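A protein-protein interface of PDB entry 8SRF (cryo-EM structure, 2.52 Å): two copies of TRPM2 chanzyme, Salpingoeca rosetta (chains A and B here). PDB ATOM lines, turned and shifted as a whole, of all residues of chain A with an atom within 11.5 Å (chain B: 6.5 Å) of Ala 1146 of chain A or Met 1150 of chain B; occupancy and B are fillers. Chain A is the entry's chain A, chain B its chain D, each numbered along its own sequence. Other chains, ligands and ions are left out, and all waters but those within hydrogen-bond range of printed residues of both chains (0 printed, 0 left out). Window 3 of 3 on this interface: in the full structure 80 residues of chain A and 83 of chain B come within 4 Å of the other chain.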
ATOM      1  N   LYS A1137      -7.562  -9.544  13.235  1.00  0.00           N
ATOM      2  CA  LYS A1137      -8.160  -9.883  14.538  1.00  0.00           C
ATOM      3  C   LYS A1137      -9.485 -10.647  14.421  1.00  0.00           C
ATOM      4  O   LYS A1137      -9.705 -11.620  15.156  1.00  0.00           O
ATOM      5  CB  LYS A1137      -8.371  -8.607  15.349  1.00  0.00           C
ATOM      6  CG  LYS A1137      -8.623  -8.840  16.825  1.00  0.00           C
ATOM      7  CD  LYS A1137      -9.209  -7.599  17.474  1.00  0.00           C
ATOM      8  CE  LYS A1137      -9.375  -7.781  18.973  1.00  0.00           C
ATOM      9  NZ  LYS A1137      -9.912  -9.127  19.309  1.00  0.00           N
ATOM     10  N   MET A1138     -10.379 -10.186  13.525  1.00  0.00           N
ATOM     11  CA  MET A1138     -11.675 -10.818  13.256  1.00  0.00           C
ATOM     12  C   MET A1138     -11.503 -12.210  12.636  1.00  0.00           C
ATOM     13  O   MET A1138     -12.242 -13.145  12.994  1.00  0.00           O
ATOM     14  CB  MET A1138     -12.551  -9.862  12.441  1.00  0.00           C
ATOM     15  CG  MET A1138     -13.929 -10.370  12.072  1.00  0.00           C
ATOM     16  SD  MET A1138     -14.771  -9.190  11.009  1.00  0.00           S
ATOM     17  CE  MET A1138     -13.824  -9.354   9.523  1.00  0.00           C
ATOM     18  N   THR A1139     -10.521 -12.333  11.712  1.00  0.00           N
ATOM     19  CA  THR A1139     -10.141 -13.585  11.047  1.00  0.00           C
ATOM     20  C   THR A1139      -9.612 -14.597  12.068  1.00  0.00           C
ATOM     21  O   THR A1139      -9.974 -15.785  12.018  1.00  0.00           O
ATOM     22  CB  THR A1139      -9.096 -13.260   9.965  1.00  0.00           C
ATOM     23  OG1 THR A1139      -9.693 -12.411   8.979  1.00  0.00           O
ATOM     24  CG2 THR A1139      -8.560 -14.497   9.249  1.00  0.00           C
ATOM     25  N   ASN A1140      -8.808 -14.097  13.030  1.00  0.00           N
ATOM     26  CA  ASN A1140      -8.219 -14.862  14.135  1.00  0.00           C
ATOM     27  C   ASN A1140      -9.300 -15.434  15.063  1.00  0.00           C
ATOM     28  O   ASN A1140      -9.221 -16.615  15.442  1.00  0.00           O
ATOM     29  CB  ASN A1140      -7.272 -13.934  14.900  1.00  0.00           C
ATOM     30  CG  ASN A1140      -6.707 -14.535  16.172  1.00  0.00           C
ATOM     31  OD1 ASN A1140      -6.375 -15.723  16.262  1.00  0.00           O
ATOM     32  ND2 ASN A1140      -6.691 -13.710  17.211  1.00  0.00           N
ATOM     33  N   ASP A1141     -10.269 -14.578  15.477  1.00  0.00           N
ATOM     34  CA  ASP A1141     -11.402 -14.997  16.324  1.00  0.00           C
ATOM     35  C   ASP A1141     -12.296 -16.020  15.622  1.00  0.00           C
ATOM     36  O   ASP A1141     -12.842 -16.921  16.282  1.00  0.00           O
ATOM     37  CB  ASP A1141     -12.233 -13.798  16.789  1.00  0.00           C
ATOM     38  CG  ASP A1141     -11.421 -12.787  17.567  1.00  0.00           C
ATOM     39  OD1 ASP A1141     -10.267 -13.096  17.931  1.00  0.00           O
ATOM     40  OD2 ASP A1141     -11.934 -11.674  17.807  1.00  0.00           O
ATOM     41  N   ASN A1142     -12.501 -15.838  14.299  1.00  0.00           N
ATOM     42  CA  ASN A1142     -13.279 -16.770  13.476  1.00  0.00           C
ATOM     43  C   ASN A1142     -12.607 -18.144  13.391  1.00  0.00           C
ATOM     44  O   ASN A1142     -13.297 -19.172  13.419  1.00  0.00           O
ATOM     45  CB  ASN A1142     -13.506 -16.191  12.082  1.00  0.00           C
ATOM     46  CG  ASN A1142     -14.586 -15.132  12.060  1.00  0.00           C
ATOM     47  OD1 ASN A1142     -15.422 -15.066  12.960  1.00  0.00           O
ATOM     48  ND2 ASN A1142     -14.576 -14.298  11.029  1.00  0.00           N
ATOM     49  N   VAL A1143     -11.268 -18.165  13.254  1.00  0.00           N
ATOM     50  CA  VAL A1143     -10.493 -19.412  13.201  1.00  0.00           C
ATOM     51  C   VAL A1143     -10.512 -20.137  14.563  1.00  0.00           C
ATOM     52  O   VAL A1143     -10.620 -21.377  14.607  1.00  0.00           O
ATOM     53  CB  VAL A1143      -9.074 -19.084  12.664  1.00  0.00           C
ATOM     54  CG1 VAL A1143      -8.010 -20.136  12.928  1.00  0.00           C
ATOM     55  CG2 VAL A1143      -9.133 -18.941  11.156  1.00  0.00           C
ATOM     56  N   VAL A1144     -10.488 -19.367  15.680  1.00  0.00           N
ATOM     57  CA  VAL A1144     -10.615 -19.902  17.056  1.00  0.00           C
ATOM     58  C   VAL A1144     -11.994 -20.548  17.299  1.00  0.00           C
ATOM     59  O   VAL A1144     -12.085 -21.679  17.829  1.00  0.00           O
ATOM     60  CB  VAL A1144     -10.278 -18.786  18.074  1.00  0.00           C
ATOM     61  CG1 VAL A1144     -10.756 -19.080  19.496  1.00  0.00           C
ATOM     62  CG2 VAL A1144      -8.774 -18.606  18.142  1.00  0.00           C
ATOM     63  N   GLN A1145     -13.073 -19.843  16.879  1.00  0.00           N
ATOM     64  CA  GLN A1145     -14.451 -20.355  16.934  1.00  0.00           C
ATOM     65  C   GLN A1145     -14.658 -21.580  16.037  1.00  0.00           C
ATOM     66  O   GLN A1145     -15.416 -22.503  16.398  1.00  0.00           O
ATOM     67  CB  GLN A1145     -15.417 -19.244  16.526  1.00  0.00           C
ATOM     68  CG  GLN A1145     -16.866 -19.471  16.907  1.00  0.00           C
ATOM     69  CD  GLN A1145     -17.748 -18.313  16.491  1.00  0.00           C
ATOM     70  OE1 GLN A1145     -17.261 -17.289  16.014  1.00  0.00           O
ATOM     71  NE2 GLN A1145     -19.056 -18.471  16.660  1.00  0.00           N
ATOM     72  N   ALA A1146     -13.956 -21.597  14.883  1.00  0.00           N
ATOM     73  CA  ALA A1146     -13.937 -22.731  13.961  1.00  0.00           C
ATOM     74  C   ALA A1146     -13.308 -23.973  14.584  1.00  0.00           C
ATOM     75  O   ALA A1146     -13.878 -25.056  14.451  1.00  0.00           O
ATOM     76  CB  ALA A1146     -13.220 -22.356  12.665  1.00  0.00           C
ATOM     77  N   MET A1147     -12.172 -23.808  15.312  1.00  0.00           N
ATOM     78  CA  MET A1147     -11.517 -24.887  16.082  1.00  0.00           C
ATOM     79  C   MET A1147     -12.403 -25.458  17.193  1.00  0.00           C
ATOM     80  O   MET A1147     -12.299 -26.665  17.485  1.00  0.00           O
ATOM     81  CB  MET A1147     -10.165 -24.443  16.647  1.00  0.00           C
ATOM     82  CG  MET A1147      -9.099 -24.212  15.584  1.00  0.00           C
ATOM     83  SD  MET A1147      -7.479 -23.711  16.203  1.00  0.00           S
ATOM     84  CE  MET A1147      -7.916 -22.595  17.530  1.00  0.00           C
ATOM     85  N   GLY A1148     -13.141 -24.573  17.902  1.00  0.00           N
ATOM     86  CA  GLY A1148     -14.118 -24.999  18.920  1.00  0.00           C
ATOM     87  C   GLY A1148     -15.210 -25.891  18.333  1.00  0.00           C
ATOM     88  O   GLY A1148     -15.613 -26.907  18.941  1.00  0.00           O
ATOM     89  N   MET A1149     -15.716 -25.490  17.154  1.00  0.00           N
ATOM     90  CA  MET A1149     -16.717 -26.268  16.423  1.00  0.00           C
ATOM     91  C   MET A1149     -16.130 -27.597  15.915  1.00  0.00           C
ATOM     92  O   MET A1149     -16.853 -28.598  15.842  1.00  0.00           O
ATOM     93  CB  MET A1149     -17.323 -25.441  15.301  1.00  0.00           C
ATOM     94  CG  MET A1149     -18.201 -24.295  15.727  1.00  0.00           C
ATOM     95  SD  MET A1149     -18.693 -23.405  14.248  1.00  0.00           S
ATOM     96  CE  MET A1149     -19.831 -24.601  13.566  1.00  0.00           C
ATOM     97  N   MET A1150     -14.830 -27.608  15.590  1.00  0.00           N
ATOM     98  CA  MET A1150     -14.159 -28.864  15.151  1.00  0.00           C
ATOM     99  C   MET A1150     -14.065 -29.810  16.350  1.00  0.00           C
ATOM    100  O   MET A1150     -14.235 -31.024  16.149  1.00  0.00           O
ATOM    101  CB  MET A1150     -12.750 -28.580  14.624  1.00  0.00           C
ATOM    102  CG  MET A1150     -12.737 -27.812  13.321  1.00  0.00           C
ATOM    103  SD  MET A1150     -11.103 -27.787  12.555  1.00  0.00           S
ATOM    104  CE  MET A1150     -10.823 -29.546  12.375  1.00  0.00           C
ATOM    105  N   ASP A1151     -13.773 -29.277  17.537  1.00  0.00           N
ATOM    106  CA  ASP A1151     -13.738 -30.083  18.766  1.00  0.00           C
ATOM    107  C   ASP A1151     -15.074 -30.794  18.977  1.00  0.00           C
ATOM    108  O   ASP A1151     -15.094 -31.975  19.378  1.00  0.00           O
ATOM    109  CB  ASP A1151     -13.401 -29.223  19.986  1.00  0.00           C
ATOM    110  CG  ASP A1151     -11.964 -28.744  19.998  1.00  0.00           C
ATOM    111  OD1 ASP A1151     -11.063 -29.557  19.718  1.00  0.00           O
ATOM    112  OD2 ASP A1151     -11.736 -27.555  20.301  1.00  0.00           O
ATOM    113  N   GLN A1152     -16.185 -30.056  18.745  1.00  0.00           N
ATOM    114  CA  GLN A1152     -17.545 -30.624  18.778  1.00  0.00           C
ATOM    115  C   GLN A1152     -17.741 -31.722  17.714  1.00  0.00           C
ATOM    116  O   GLN A1152     -18.388 -32.751  17.987  1.00  0.00           O
ATOM    117  CB  GLN A1152     -18.585 -29.522  18.583  1.00  0.00           C
ATOM    118  CG  GLN A1152     -18.650 -28.490  19.685  1.00  0.00           C
ATOM    119  CD  GLN A1152     -19.200 -27.168  19.189  1.00  0.00           C
ATOM    120  OE1 GLN A1152     -20.193 -27.135  18.462  1.00  0.00           O
ATOM    121  NE2 GLN A1152     -18.559 -26.071  19.576  1.00  0.00           N
ATOM    122  N   LEU A1153     -17.229 -31.471  16.480  1.00  0.00           N
ATOM    123  CA  LEU A1153     -17.278 -32.425  15.352  1.00  0.00           C
ATOM    124  C   LEU A1153     -16.513 -33.718  15.659  1.00  0.00           C
ATOM    125  O   LEU A1153     -16.980 -34.817  15.326  1.00  0.00           O
ATOM    126  CB  LEU A1153     -16.715 -31.809  14.065  1.00  0.00           C
ATOM    127  CG  LEU A1153     -17.366 -30.686  13.236  1.00  0.00           C
ATOM    128  CD1 LEU A1153     -16.358 -30.151  12.223  1.00  0.00           C
ATOM    129  CD2 LEU A1153     -18.710 -30.977  12.587  1.00  0.00           C
ATOM    130  N   LEU A1154     -15.315 -33.580  16.266  1.00  0.00           N
ATOM    131  CA  LEU A1154     -14.447 -34.705  16.637  1.00  0.00           C
ATOM    132  C   LEU A1154     -15.080 -35.541  17.748  1.00  0.00           C
ATOM    133  O   LEU A1154     -14.892 -36.772  17.787  1.00  0.00           O
ATOM    134  CB  LEU A1154     -13.072 -34.183  17.050  1.00  0.00           C
ATOM    135  CG  LEU A1154     -11.932 -35.199  17.116  1.00  0.00           C
ATOM    136  CD1 LEU A1154     -11.498 -35.600  15.717  1.00  0.00           C
ATOM    137  CD2 LEU A1154     -10.764 -34.624  17.896  1.00  0.00           C
ATOM    138  N   GLU A1155     -15.776 -34.854  18.683  1.00  0.00           N
ATOM    139  CA  GLU A1155     -16.567 -35.489  19.743  1.00  0.00           C
ATOM    140  C   GLU A1155     -17.690 -36.345  19.147  1.00  0.00           C
ATOM    141  O   GLU A1155     -17.917 -37.483  19.599  1.00  0.00           O
ATOM    142  CB  GLU A1155     -17.105 -34.411  20.697  1.00  0.00           C
ATOM    143  CG  GLU A1155     -18.355 -34.761  21.501  1.00  0.00           C
ATOM    144  CD  GLU A1155     -18.120 -35.833  22.550  1.00  0.00           C
ATOM    145  OE1 GLU A1155     -16.995 -35.933  23.090  1.00  0.00           O
ATOM    146  OE2 GLU A1155     -19.080 -36.578  22.838  1.00  0.00           O
ATOM    147  N   HIS A1156     -18.297 -35.826  18.081  1.00  0.00           N
ATOM    148  CA  HIS A1156     -19.414 -36.544  17.424  1.00  0.00           C
ATOM    149  C   HIS A1156     -18.873 -37.739  16.652  1.00  0.00           C
ATOM    150  O   HIS A1156     -19.598 -38.725  16.556  1.00  0.00           O
ATOM    151  CB  HIS A1156     -20.135 -35.633  16.435  1.00  0.00           C
ATOM    152  CG  HIS A1156     -21.200 -34.782  17.031  1.00  0.00           C
ATOM    153  ND1 HIS A1156     -21.213 -33.411  16.878  1.00  0.00           N
ATOM    154  CD2 HIS A1156     -22.294 -35.093  17.756  1.00  0.00           C
ATOM    155  CE1 HIS A1156     -22.263 -32.912  17.494  1.00  0.00           C
ATOM    156  NE2 HIS A1156     -22.943 -33.923  18.039  1.00  0.00           N
ATOM    157  N   MET A1157     -17.662 -37.664  16.118  1.00  0.00           N
ATOM    158  CA  MET A1157     -17.167 -38.873  15.415  1.00  0.00           C
ATOM    159  C   MET A1157     -16.769 -39.947  16.434  1.00  0.00           C
ATOM    160  O   MET A1157     -17.034 -41.130  16.159  1.00  0.00           O
ATOM    161  CB  MET A1157     -15.991 -38.549  14.495  1.00  0.00           C
ATOM    162  CG  MET A1157     -16.392 -37.676  13.326  1.00  0.00           C
ATOM    163  SD  MET A1157     -14.913 -37.302  12.384  1.00  0.00           S
ATOM    164  CE  MET A1157     -15.653 -36.241  11.144  1.00  0.00           C
ATOM    165  N   VAL B1143     -12.581 -18.027   5.209  1.00  0.00           N
ATOM    166  CA  VAL B1143     -12.789 -18.560   6.562  1.00  0.00           C
ATOM    167  C   VAL B1143     -14.273 -18.469   6.973  1.00  0.00           C
ATOM    168  O   VAL B1143     -14.803 -19.404   7.604  1.00  0.00           O
ATOM    169  CB  VAL B1143     -11.807 -17.841   7.527  1.00  0.00           C
ATOM    170  CG1 VAL B1143     -12.147 -17.938   9.005  1.00  0.00           C
ATOM    171  CG2 VAL B1143     -10.431 -18.460   7.389  1.00  0.00           C
ATOM    172  N   GLN B1145     -16.912 -18.504   4.726  1.00  0.00           N
ATOM    173  CA  GLN B1145     -17.522 -19.556   3.899  1.00  0.00           C
ATOM    174  C   GLN B1145     -17.237 -20.963   4.435  1.00  0.00           C
ATOM    175  O   GLN B1145     -18.105 -21.856   4.353  1.00  0.00           O
ATOM    176  CB  GLN B1145     -17.006 -19.432   2.466  1.00  0.00           C
ATOM    177  CG  GLN B1145     -17.819 -20.164   1.418  1.00  0.00           C
ATOM    178  CD  GLN B1145     -17.257 -19.967   0.026  1.00  0.00           C
ATOM    179  OE1 GLN B1145     -16.321 -19.193  -0.171  1.00  0.00           O
ATOM    180  NE2 GLN B1145     -17.818 -20.674  -0.947  1.00  0.00           N
ATOM    181  N   ALA B1146     -16.029 -21.146   5.012  1.00  0.00           N
ATOM    182  CA  ALA B1146     -15.627 -22.383   5.679  1.00  0.00           C
ATOM    183  C   ALA B1146     -16.473 -22.676   6.914  1.00  0.00           C
ATOM    184  O   ALA B1146     -16.911 -23.815   7.075  1.00  0.00           O
ATOM    185  CB  ALA B1146     -14.143 -22.339   6.040  1.00  0.00           C
ATOM    186  N   MET B1147     -16.752 -21.640   7.748  1.00  0.00           N
ATOM    187  CA  MET B1147     -17.661 -21.733   8.910  1.00  0.00           C
ATOM    188  C   MET B1147     -19.099 -22.091   8.525  1.00  0.00           C
ATOM    189  O   MET B1147     -19.780 -22.780   9.309  1.00  0.00           O
ATOM    190  CB  MET B1147     -17.633 -20.459   9.759  1.00  0.00           C
ATOM    191  CG  MET B1147     -16.316 -20.234  10.490  1.00  0.00           C
ATOM    192  SD  MET B1147     -16.243 -18.755  11.524  1.00  0.00           S
ATOM    193  CE  MET B1147     -17.124 -17.560  10.528  1.00  0.00           C
ATOM    194  N   GLY B1148     -19.598 -21.501   7.415  1.00  0.00           N
ATOM    195  CA  GLY B1148     -20.924 -21.843   6.869  1.00  0.00           C
ATOM    196  C   GLY B1148     -21.030 -23.319   6.492  1.00  0.00           C
ATOM    197  O   GLY B1148     -22.056 -23.984   6.755  1.00  0.00           O
ATOM    198  N   MET B1149     -19.969 -23.829   5.842  1.00  0.00           N
ATOM    199  CA  MET B1149     -19.879 -25.242   5.472  1.00  0.00           C
ATOM    200  C   MET B1149     -19.764 -26.139   6.718  1.00  0.00           C
ATOM    201  O   MET B1149     -20.266 -27.270   6.707  1.00  0.00           O
ATOM    202  CB  MET B1149     -18.738 -25.468   4.494  1.00  0.00           C
ATOM    203  CG  MET B1149     -18.926 -24.891   3.117  1.00  0.00           C
ATOM    204  SD  MET B1149     -17.414 -25.177   2.193  1.00  0.00           S
ATOM    205  CE  MET B1149     -17.560 -26.940   1.954  1.00  0.00           C
ATOM    206  N   MET B1150     -19.130 -25.631   7.782  1.00  0.00           N
ATOM    207  CA  MET B1150     -19.026 -26.400   9.054  1.00  0.00           C
ATOM    208  C   MET B1150     -20.417 -26.488   9.685  1.00  0.00           C
ATOM    209  O   MET B1150     -20.736 -27.548  10.247  1.00  0.00           O
ATOM    210  CB  MET B1150     -18.073 -25.715  10.036  1.00  0.00           C
ATOM    211  CG  MET B1150     -16.626 -25.749   9.596  1.00  0.00           C
ATOM    212  SD  MET B1150     -15.495 -25.246  10.910  1.00  0.00           S
ATOM    213  CE  MET B1150     -15.915 -26.462  12.156  1.00  0.00           C
ATOM    214  N   ASP B1151     -21.195 -25.406   9.620  1.00  0.00           N
ATOM    215  CA  ASP B1151     -22.577 -25.408  10.121  1.00  0.00           C
ATOM    216  C   ASP B1151     -23.389 -26.512   9.444  1.00  0.00           C
ATOM    217  O   ASP B1151     -24.190 -27.194  10.113  1.00  0.00           O
ATOM    218  CB  ASP B1151     -23.250 -24.051   9.904  1.00  0.00           C
ATOM    219  CG  ASP B1151     -22.695 -22.962  10.799  1.00  0.00           C
ATOM    220  OD1 ASP B1151     -22.506 -23.218  12.002  1.00  0.00           O
ATOM    221  OD2 ASP B1151     -22.460 -21.843  10.298  1.00  0.00           O
ATOM    222  N   GLN B1152     -23.208 -26.652   8.109  1.00  0.00           N
ATOM    223  CA  GLN B1152     -23.815 -27.746   7.329  1.00  0.00           C
ATOM    224  C   GLN B1152     -23.330 -29.132   7.800  1.00  0.00           C
ATOM    225  O   GLN B1152     -24.130 -30.085   7.869  1.00  0.00           O
ATOM    226  CB  GLN B1152     -23.511 -27.568   5.842  1.00  0.00           C
ATOM    227  CG  GLN B1152     -24.124 -26.347   5.198  1.00  0.00           C
ATOM    228  CD  GLN B1152     -23.340 -25.897   3.982  1.00  0.00           C
ATOM    229  OE1 GLN B1152     -22.949 -26.715   3.149  1.00  0.00           O
ATOM    230  NE2 GLN B1152     -23.102 -24.595   3.871  1.00  0.00           N
ATOM    231  N   LEU B1153     -22.003 -29.254   8.066  1.00  0.00           N
ATOM    232  CA  LEU B1153     -21.370 -30.489   8.573  1.00  0.00           C
ATOM    233  C   LEU B1153     -21.917 -30.895   9.947  1.00  0.00           C
ATOM    234  O   LEU B1153     -22.156 -32.084  10.200  1.00  0.00           O
ATOM    235  CB  LEU B1153     -19.846 -30.345   8.668  1.00  0.00           C
ATOM    236  CG  LEU B1153     -18.867 -30.245   7.484  1.00  0.00           C
ATOM    237  CD1 LEU B1153     -17.496 -29.806   7.991  1.00  0.00           C
ATOM    238  CD2 LEU B1153     -18.760 -31.442   6.553  1.00  0.00           C
ATOM    239  N   LEU B1154     -22.083 -29.903  10.846  1.00  0.00           N
ATOM    240  CA  LEU B1154     -22.596 -30.104  12.207  1.00  0.00           C
ATOM    241  C   LEU B1154     -24.065 -30.524  12.180  1.00  0.00           C
ATOM    242  O   LEU B1154     -24.506 -31.303  13.046  1.00  0.00           O
ATOM    243  CB  LEU B1154     -22.398 -28.830  13.028  1.00  0.00           C
ATOM    244  CG  LEU B1154     -22.527 -28.953  14.546  1.00  0.00           C
ATOM    245  CD1 LEU B1154     -21.317 -29.664  15.125  1.00  0.00           C
ATOM    246  CD2 LEU B1154     -22.692 -27.578  15.170  1.00  0.00           C
ATOM    247  N   GLU B1155     -24.827 -29.953  11.219  1.00  0.00           N
ATOM    248  CA  GLU B1155     -26.218 -30.332  10.947  1.00  0.00           C
ATOM    249  C   GLU B1155     -26.310 -31.801  10.524  1.00  0.00           C
ATOM    250  O   GLU B1155     -27.197 -32.537  11.001  1.00  0.00           O
ATOM    251  CB  GLU B1155     -26.809 -29.387   9.890  1.00  0.00           C
ATOM    252  CG  GLU B1155     -27.990 -29.912   9.077  1.00  0.00           C
ATOM    253  CD  GLU B1155     -29.258 -30.087   9.895  1.00  0.00           C
ATOM    254  OE1 GLU B1155     -29.471 -29.336  10.872  1.00  0.00           O
ATOM    255  OE2 GLU B1155     -30.049 -30.988   9.545  1.00  0.00           O
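The backbone carbonyl oxygen of Asn 1142 of chain A sits close to the side-chain sulfur of Met 1147 of chain B (3.5 Å).
ND2 of Asn 1142 of chain A lies close to O of Met 1138 of chain A.
Asn 1142 of chain A touches Val 1143 of chain B (CB to CG1, 3.8 Å). Val 1143 of chain A touches Val 1143 of chain B (CG2 to CG1, 3.8 Å). O of Ala 1146 of chain A touches CE of Met 1150 of chain B, 3.4 Å away. Met 1149 of chain A touches Met 1150 of chain B (CB to CE, 3.6 Å). CE of Met 1149 of chain A touches OD1 of Asp 1151 of chain B, at 3.4 Å. Met 1150 of chain A touches Met 1150 of chain B. CD1 of Leu 1153 of chain A touches CE of Met 1150 of chain B, at 3.7 Å. Leu 1153 of chain A touches Leu 1154 of chain B.
Printed residues of chain B within 4 Å of Asn 1142 of chain A: Val 1143 (3.8 Å) and Met 1147 (3.5 Å). Of the printed residues of chain B, Val 1143 of chain A touches Val 1143. Ala 1146 of chain A touches one residue of chain B. Of the printed residues of chain B, Leu 1153 of chain A touches Met 1150 (3.7 Å) and Leu 1154 (3.9 Å). No residue of chain A comes within 4 Å of Ala 1146 of chain B. Met 1147 of chain B touches just one residue of chain A: Asn 1142. Gly 1148 of chain B touches none of the printed residues of chain A. No residue of chain A comes within 4 Å of Met 1149 of chain B. Of chain A, only Ala 1146, Met 1149, Met 1150 and Leu 1153 come within 4 Å of Met 1150 of chain B. Asp 1151 of chain B touches one residue of chain A. No residue of chain A comes within 4 Å of Gln 1152 of chain B. No residue of chain A comes within 4 Å of Leu 1153 of chain B. Of chain A, only Leu 1153 (3.9 Å) comes within 4 Å of Leu 1154 of chain B. The nearest printed residue of chain B that does not touch Asn 1142 of chain A is Met 1150 of chain B (6.9 Å).
Hydrophobic or aromatic side chains of chain B within 4 Å of the printed part of chain A: Val 1143, Met 1147, Met 1150 and Leu 1154. Among the printed residues, 9 pairs touch across the chains. Among the printed residues, no Asp or Glu carboxylate lies within 4 Å of a Lys or Arg side-chain nitrogen of the other chain.
Met 1149 of chain A touches Asp 1151 of chain B, but with the chains exchanged Asp 1151 of chain A does not touch Met 1149 of chain B (12.8 Å). Met 1150 of chain A touches its own counterpart, Met 1150 of chain B. Leu 1153 of chain A touches Met 1150 of chain B, but with the chains exchanged Met 1150 of chain A does not touch Leu 1153 of chain B (7.4 Å). Leu 1153 of chain A touches Leu 1154 of chain B, but with the chains exchanged Leu 1154 of chain A does not touch Leu 1153 of chain B (9.3 Å).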
